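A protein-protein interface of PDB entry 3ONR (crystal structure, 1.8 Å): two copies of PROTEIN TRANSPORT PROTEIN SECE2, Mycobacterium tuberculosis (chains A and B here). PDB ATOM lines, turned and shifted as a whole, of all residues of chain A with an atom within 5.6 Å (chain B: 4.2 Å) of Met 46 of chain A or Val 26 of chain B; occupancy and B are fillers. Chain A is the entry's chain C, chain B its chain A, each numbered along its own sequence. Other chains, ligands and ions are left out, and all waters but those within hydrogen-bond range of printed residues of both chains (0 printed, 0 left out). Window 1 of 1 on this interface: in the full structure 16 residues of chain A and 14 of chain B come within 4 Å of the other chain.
N of Ala 39 of chain B is in hydrogen-bond range of O of Met 46 of chain A, 2.9 Å away.
The indole nitrogen of Trp 18 of chain A is in hydrogen-bond range of the backbone carbonyl oxygen of Asp 45 of chain A (3.1 Å). The backbone carbonyl oxygen of Arg 57 of chain A sits at hydrogen-bond distance from the indole nitrogen of Trp 18 of chain A (3.0 Å). NE of Arg 57 of chain A is in salt-bridge range of OD2 of Asp 45 of chain A.
Among the printed residues, merely in contact across the chains: Asp 45 of chain A with Ala 39 of chain B (3.3 Å), Met 46 of chain A with Val 38 of chain B (3.3 Å), Ile 54 of chain A with Ala 23 of chain B (3.6 Å), Met 46 of chain A with Ala 22 of chain B (3.6 Å), Val 48 of chain A with Arg 30 of chain B (3.7 Å), Tyr 56 of chain A with Ala 23 of chain B (3.8 Å), Val 48 of chain A with Val 26 of chain B (3.8 Å), Arg 57 of chain A with Val 38 of chain B (3.9 Å), Met 46 of chain A with Val 26 of chain B (3.9 Å), Met 46 of chain A with Ala 23 of chain B (3.97 Å) and Trp 18 of chain A with Ala 22 of chain B (3.98 Å).
Printed residues of chain B within 4 Å of Asp 45 of chain A: Ala 39. Met 46 of chain A touches just these residues of chain B: Ala 22 (3.6 Å), Ala 23 (3.97 Å), Val 26 (3.9 Å), Val 38 (3.3 Å) and Ala 39 (2.9 Å). Printed residues of chain B within 4 Å of Val 48 of chain A: Val 26 (3.8 Å) and Arg 30 (3.7 Å). Printed residues of chain B within 4 Å of Ile 54 of chain A: Ala 23 (3.6 Å). Thr 55 of chain A touches none of the printed residues of chain B. Printed residues of chain B within 4 Å of Arg 57 of chain A: Val 38 (3.9 Å). Of the printed residues of chain A, Ala 22 of chain B touches Trp 18 (3.98 Å) and Met 46 (3.6 Å). Val 26 of chain B touches two residues of chain A. The nearest printed residue of chain B that does not touch Met 46 of chain A is Leu 60 of chain B (4.6 Å).
Hydrophobic or aromatic side chains of chain B that line the printed part of chain A: Ala 22, Ala 23, Val 26 and Val 38. Of the 10 printed residues of chain A, 7 touch a printed residue of chain B. Hydrophobic or aromatic side chains of chain A within 4 Å of the printed part of chain B: Trp 18, Met 46, Val 48, Ile 54 and Tyr 56. Among the printed residues, no Asp or Glu carboxylate lies within 4 Å of a Lys or Arg side-chain nitrogen of the other chain.
No position is printed for both chains.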
ATOM      1  N   TRP A  18      22.253  -7.554  28.277  1.00  0.00           N
ATOM      2  CA  TRP A  18      22.016  -7.321  29.660  1.00  0.00           C
ATOM      3  C   TRP A  18      22.549  -8.425  30.589  1.00  0.00           C
ATOM      4  O   TRP A  18      22.881  -8.115  31.744  1.00  0.00           O
ATOM      5  CB  TRP A  18      20.494  -7.105  29.927  1.00  0.00           C
ATOM      6  CG  TRP A  18      20.029  -5.750  29.450  1.00  0.00           C
ATOM      7  CD1 TRP A  18      20.454  -4.505  29.947  1.00  0.00           C
ATOM      8  CD2 TRP A  18      19.056  -5.453  28.436  1.00  0.00           C
ATOM      9  NE1 TRP A  18      19.747  -3.497  29.326  1.00  0.00           N
ATOM     10  CE2 TRP A  18      18.918  -4.034  28.385  1.00  0.00           C
ATOM     11  CE3 TRP A  18      18.251  -6.235  27.575  1.00  0.00           C
ATOM     12  CZ2 TRP A  18      18.051  -3.393  27.482  1.00  0.00           C
ATOM     13  CZ3 TRP A  18      17.409  -5.591  26.705  1.00  0.00           C
ATOM     14  CH2 TRP A  18      17.299  -4.184  26.676  1.00  0.00           C
ATOM     15  N   GLN A  44      16.346  -1.703  33.660  1.00  0.00           N
ATOM     16  CA  GLN A  44      17.192  -1.943  32.483  1.00  0.00           C
ATOM     17  C   GLN A  44      17.043  -0.763  31.533  1.00  0.00           C
ATOM     18  O   GLN A  44      15.954  -0.192  31.373  1.00  0.00           O
ATOM     19  CB  GLN A  44      16.760  -3.213  31.700  1.00  0.00           C
ATOM     20  CG  GLN A  44      17.095  -4.509  32.503  1.00  0.00           C
ATOM     21  CD  GLN A  44      16.502  -5.724  31.814  1.00  0.00           C
ATOM     22  OE1 GLN A  44      17.199  -6.506  31.111  1.00  0.00           O
ATOM     23  NE2 GLN A  44      15.187  -5.834  31.926  1.00  0.00           N
ATOM     24  N   ASP A  45      18.141  -0.360  30.897  1.00  0.00           N
ATOM     25  CA  ASP A  45      18.026   0.652  29.858  1.00  0.00           C
ATOM     26  C   ASP A  45      19.153   0.488  28.807  1.00  0.00           C
ATOM     27  O   ASP A  45      19.925  -0.473  28.843  1.00  0.00           O
ATOM     28  CB  ASP A  45      17.957   2.062  30.486  1.00  0.00           C
ATOM     29  CG  ASP A  45      19.312   2.599  31.008  1.00  0.00           C
ATOM     30  OD1 ASP A  45      19.339   3.698  31.623  1.00  0.00           O
ATOM     31  OD2 ASP A  45      20.373   2.036  30.686  1.00  0.00           O
ATOM     32  N   MET A  46      19.253   1.452  27.883  1.00  0.00           N
ATOM     33  CA  MET A  46      20.387   1.437  26.958  1.00  0.00           C
ATOM     34  C   MET A  46      20.809   2.826  26.806  1.00  0.00           C
ATOM     35  O   MET A  46      19.945   3.735  26.751  1.00  0.00           O
ATOM     36  CB  MET A  46      19.911   1.038  25.572  1.00  0.00           C
ATOM     37  CG  MET A  46      19.453  -0.332  25.486  1.00  0.00           C
ATOM     38  SD  MET A  46      18.067  -0.408  24.355  1.00  0.00           S
ATOM     39  CE  MET A  46      18.910  -1.033  23.011  1.00  0.00           C
ATOM     40  N   ALA A  47      22.121   3.020  26.629  1.00  0.00           N
ATOM     41  CA  ALA A  47      22.655   4.314  26.243  1.00  0.00           C
ATOM     42  C   ALA A  47      22.883   4.116  24.775  1.00  0.00           C
ATOM     43  O   ALA A  47      23.243   3.010  24.324  1.00  0.00           O
ATOM     44  CB  ALA A  47      24.016   4.598  26.949  1.00  0.00           C
ATOM     45  N   VAL A  48      22.715   5.188  24.009  1.00  0.00           N
ATOM     46  CA  VAL A  48      22.927   5.127  22.602  1.00  0.00           C
ATOM     47  C   VAL A  48      23.792   6.364  22.259  1.00  0.00           C
ATOM     48  O   VAL A  48      23.417   7.505  22.581  1.00  0.00           O
ATOM     49  CB  VAL A  48      21.552   5.208  21.837  1.00  0.00           C
ATOM     50  CG1 VAL A  48      21.723   4.688  20.408  1.00  0.00           C
ATOM     51  CG2 VAL A  48      20.437   4.382  22.556  1.00  0.00           C
ATOM     52  N   ILE A  54      25.186   1.013  20.758  1.00  0.00           N
ATOM     53  CA  ILE A  54      24.348   0.733  21.942  1.00  0.00           C
ATOM     54  C   ILE A  54      25.141   0.165  23.132  1.00  0.00           C
ATOM     55  O   ILE A  54      26.039  -0.661  22.961  1.00  0.00           O
ATOM     56  CB  ILE A  54      23.124  -0.217  21.596  1.00  0.00           C
ATOM     57  CG1 ILE A  54      22.192   0.506  20.594  1.00  0.00           C
ATOM     58  CG2 ILE A  54      22.338  -0.674  22.912  1.00  0.00           C
ATOM     59  CD1 ILE A  54      21.016  -0.391  20.130  1.00  0.00           C
ATOM     60  N   THR A  55      24.805   0.619  24.341  1.00  0.00           N
ATOM     61  CA  THR A  55      25.326   0.035  25.557  1.00  0.00           C
ATOM     62  C   THR A  55      24.155  -0.377  26.406  1.00  0.00           C
ATOM     63  O   THR A  55      23.312   0.490  26.796  1.00  0.00           O
ATOM     64  CB  THR A  55      26.186   1.069  26.389  1.00  0.00           C
ATOM     65  OG1 THR A  55      27.278   1.533  25.588  1.00  0.00           O
ATOM     66  CG2 THR A  55      26.753   0.381  27.605  1.00  0.00           C
ATOM     67  N   TYR A  56      24.109  -1.672  26.744  1.00  0.00           N
ATOM     68  CA  TYR A  56      23.015  -2.212  27.590  1.00  0.00           C
ATOM     69  C   TYR A  56      23.403  -1.960  29.017  1.00  0.00           C
ATOM     70  O   TYR A  56      24.542  -2.243  29.421  1.00  0.00           O
ATOM     71  CB  TYR A  56      22.874  -3.734  27.307  1.00  0.00           C
ATOM     72  CG  TYR A  56      22.409  -3.961  25.866  1.00  0.00           C
ATOM     73  CD1 TYR A  56      23.336  -4.303  24.852  1.00  0.00           C
ATOM     74  CD2 TYR A  56      21.047  -3.743  25.506  1.00  0.00           C
ATOM     75  CE1 TYR A  56      22.909  -4.430  23.522  1.00  0.00           C
ATOM     76  CE2 TYR A  56      20.624  -3.858  24.146  1.00  0.00           C
ATOM     77  CZ  TYR A  56      21.534  -4.244  23.201  1.00  0.00           C
ATOM     78  OH  TYR A  56      21.170  -4.340  21.875  1.00  0.00           O
ATOM     79  N   ARG A  57      22.478  -1.432  29.812  1.00  0.00           N
ATOM     80  CA  ARG A  57      22.849  -1.139  31.198  1.00  0.00           C
ATOM     81  C   ARG A  57      21.770  -1.763  32.101  1.00  0.00           C
ATOM     82  O   ARG A  57      20.598  -1.840  31.711  1.00  0.00           O
ATOM     83  CB  ARG A  57      22.972   0.366  31.454  1.00  0.00           C
ATOM     84  CG  ARG A  57      23.980   1.053  30.505  1.00  0.00           C
ATOM     85  CD  ARG A  57      24.146   2.512  30.804  1.00  0.00           C
ATOM     86  NE  ARG A  57      22.876   3.239  30.859  1.00  0.00           N
ATOM     87  CZ  ARG A  57      22.803   4.575  30.921  1.00  0.00           C
ATOM     88  NH1 ARG A  57      23.930   5.323  30.897  1.00  0.00           N
ATOM     89  NH2 ARG A  57      21.623   5.194  30.959  1.00  0.00           N
ATOM     90  N   ALA B  22      15.114  -4.715  21.157  1.00  0.00           N
ATOM     91  CA  ALA B  22      15.385  -3.324  21.604  1.00  0.00           C
ATOM     92  C   ALA B  22      16.228  -2.542  20.594  1.00  0.00           C
ATOM     93  O   ALA B  22      15.924  -1.364  20.342  1.00  0.00           O
ATOM     94  CB  ALA B  22      16.094  -3.320  22.985  1.00  0.00           C
ATOM     95  N   ALA B  23      17.295  -3.148  20.065  1.00  0.00           N
ATOM     96  CA  ALA B  23      18.160  -2.451  19.096  1.00  0.00           C
ATOM     97  C   ALA B  23      17.375  -2.112  17.845  1.00  0.00           C
ATOM     98  O   ALA B  23      17.598  -1.036  17.257  1.00  0.00           O
ATOM     99  CB  ALA B  23      19.391  -3.265  18.740  1.00  0.00           C
ATOM    100  N   GLU B  24      16.440  -2.978  17.458  1.00  0.00           N
ATOM    101  CA  GLU B  24      15.606  -2.732  16.242  1.00  0.00           C
ATOM    102  C   GLU B  24      14.743  -1.489  16.476  1.00  0.00           C
ATOM    103  O   GLU B  24      14.667  -0.658  15.573  1.00  0.00           O
ATOM    104  CB  GLU B  24      14.664  -3.910  15.951  1.00  0.00           C
ATOM    105  CG  GLU B  24      15.372  -5.216  15.542  1.00  0.00           C
ATOM    106  CD  GLU B  24      15.924  -5.238  14.184  1.00  0.00           C
ATOM    107  OE1 GLU B  24      16.457  -6.303  13.810  1.00  0.00           O
ATOM    108  OE2 GLU B  24      15.802  -4.213  13.464  1.00  0.00           O
ATOM    109  N   ALA B  25      14.091  -1.443  17.640  1.00  0.00           N
ATOM    110  CA  ALA B  25      13.258  -0.269  18.050  1.00  0.00           C
ATOM    111  C   ALA B  25      14.112   1.002  18.062  1.00  0.00           C
ATOM    112  O   ALA B  25      13.730   2.008  17.454  1.00  0.00           O
ATOM    113  CB  ALA B  25      12.612  -0.468  19.398  1.00  0.00           C
ATOM    114  N   VAL B  26      15.242   0.961  18.766  1.00  0.00           N
ATOM    115  CA  VAL B  26      16.145   2.160  18.736  1.00  0.00           C
ATOM    116  C   VAL B  26      16.605   2.574  17.359  1.00  0.00           C
ATOM    117  O   VAL B  26      16.535   3.769  17.024  1.00  0.00           O
ATOM    118  CB  VAL B  26      17.390   1.968  19.638  1.00  0.00           C
ATOM    119  CG1 VAL B  26      18.395   3.080  19.396  1.00  0.00           C
ATOM    120  CG2 VAL B  26      16.942   1.822  21.126  1.00  0.00           C
ATOM    121  N   GLN B  27      17.036   1.638  16.528  1.00  0.00           N
ATOM    122  CA  GLN B  27      17.468   2.031  15.158  1.00  0.00           C
ATOM    123  C   GLN B  27      16.365   2.682  14.303  1.00  0.00           C
ATOM    124  O   GLN B  27      16.591   3.725  13.633  1.00  0.00           O
ATOM    125  CB  GLN B  27      18.075   0.837  14.478  1.00  0.00           C
ATOM    126  CG  GLN B  27      19.550   0.581  14.953  1.00  0.00           C
ATOM    127  CD  GLN B  27      20.374   1.896  15.220  1.00  0.00           C
ATOM    128  OE1 GLN B  27      20.547   2.755  14.320  1.00  0.00           O
ATOM    129  NE2 GLN B  27      20.865   2.043  16.467  1.00  0.00           N
ATOM    130  N   ARG B  28      15.160   2.086  14.383  1.00  0.00           N
ATOM    131  CA  ARG B  28      13.949   2.659  13.765  1.00  0.00           C
ATOM    132  C   ARG B  28      13.703   4.125  14.306  1.00  0.00           C
ATOM    133  O   ARG B  28      13.523   5.077  13.514  1.00  0.00           O
ATOM    134  CB  ARG B  28      12.701   1.763  14.002  1.00  0.00           C
ATOM    135  CG  ARG B  28      11.371   2.411  13.471  1.00  0.00           C
ATOM    136  CD  ARG B  28      11.460   2.720  11.927  1.00  0.00           C
ATOM    137  NE  ARG B  28      10.328   3.551  11.408  1.00  0.00           N
ATOM    138  CZ  ARG B  28      10.151   4.886  11.552  1.00  0.00           C
ATOM    139  NH1 ARG B  28      11.000   5.645  12.240  1.00  0.00           N
ATOM    140  NH2 ARG B  28       9.121   5.487  10.950  1.00  0.00           N
ATOM    141  N   ALA B  29      13.733   4.310  15.620  1.00  0.00           N
ATOM    142  CA  ALA B  29      13.619   5.645  16.223  1.00  0.00           C
ATOM    143  C   ALA B  29      14.675   6.617  15.629  1.00  0.00           C
ATOM    144  O   ALA B  29      14.385   7.768  15.222  1.00  0.00           O
ATOM    145  CB  ALA B  29      13.765   5.560  17.740  1.00  0.00           C
ATOM    146  N   ARG B  30      15.928   6.159  15.573  1.00  0.00           N
ATOM    147  CA  ARG B  30      16.957   7.019  15.031  1.00  0.00           C
ATOM    148  C   ARG B  30      16.830   7.302  13.554  1.00  0.00           C
ATOM    149  O   ARG B  30      17.508   8.209  13.035  1.00  0.00           O
ATOM    150  CB  ARG B  30      18.354   6.492  15.375  1.00  0.00           C
ATOM    151  CG  ARG B  30      18.566   6.554  16.925  1.00  0.00           C
ATOM    152  CD  ARG B  30      19.818   5.816  17.446  1.00  0.00           C
ATOM    153  NE  ARG B  30      20.841   5.645  16.419  1.00  0.00           N
ATOM    154  CZ  ARG B  30      21.658   6.583  15.949  1.00  0.00           C
ATOM    155  NH1 ARG B  30      21.623   7.828  16.408  1.00  0.00           N
ATOM    156  NH2 ARG B  30      22.514   6.259  14.985  1.00  0.00           N
ATOM    157  N   VAL B  38      19.295   7.790  25.047  1.00  0.00           N
ATOM    158  CA  VAL B  38      18.939   6.838  26.084  1.00  0.00           C
ATOM    159  C   VAL B  38      17.639   6.207  25.767  1.00  0.00           C
ATOM    160  O   VAL B  38      16.789   6.905  25.207  1.00  0.00           O
ATOM    161  CB  VAL B  38      18.955   7.438  27.522  1.00  0.00           C
ATOM    162  CG1 VAL B  38      17.848   8.425  27.755  1.00  0.00           C
ATOM    163  CG2 VAL B  38      18.789   6.328  28.540  1.00  0.00           C
ATOM    164  N   ALA B  39      17.417   4.920  26.111  1.00  0.00           N
ATOM    165  CA  ALA B  39      16.090   4.313  25.948  1.00  0.00           C
ATOM    166  C   ALA B  39      15.795   3.486  27.172  1.00  0.00           C
ATOM    167  O   ALA B  39      16.632   2.613  27.499  1.00  0.00           O
ATOM    168  CB  ALA B  39      16.025   3.387  24.761  1.00  0.00           C
ATOM    169  N   LEU B  60       9.974   0.251  25.039  1.00  0.00           N
ATOM    170  CA  LEU B  60      11.009   1.214  25.378  1.00  0.00           C
ATOM    171  C   LEU B  60      10.422   2.644  25.427  1.00  0.00           C
ATOM    172  O   LEU B  60       9.564   2.969  24.652  1.00  0.00           O
ATOM    173  CB  LEU B  60      12.074   1.266  24.317  1.00  0.00           C
ATOM    174  CG  LEU B  60      12.815  -0.085  24.004  1.00  0.00           C
ATOM    175  CD1 LEU B  60      13.769   0.108  22.887  1.00  0.00           C
ATOM    176  CD2 LEU B  60      13.576  -0.542  25.275  1.00  0.00           C
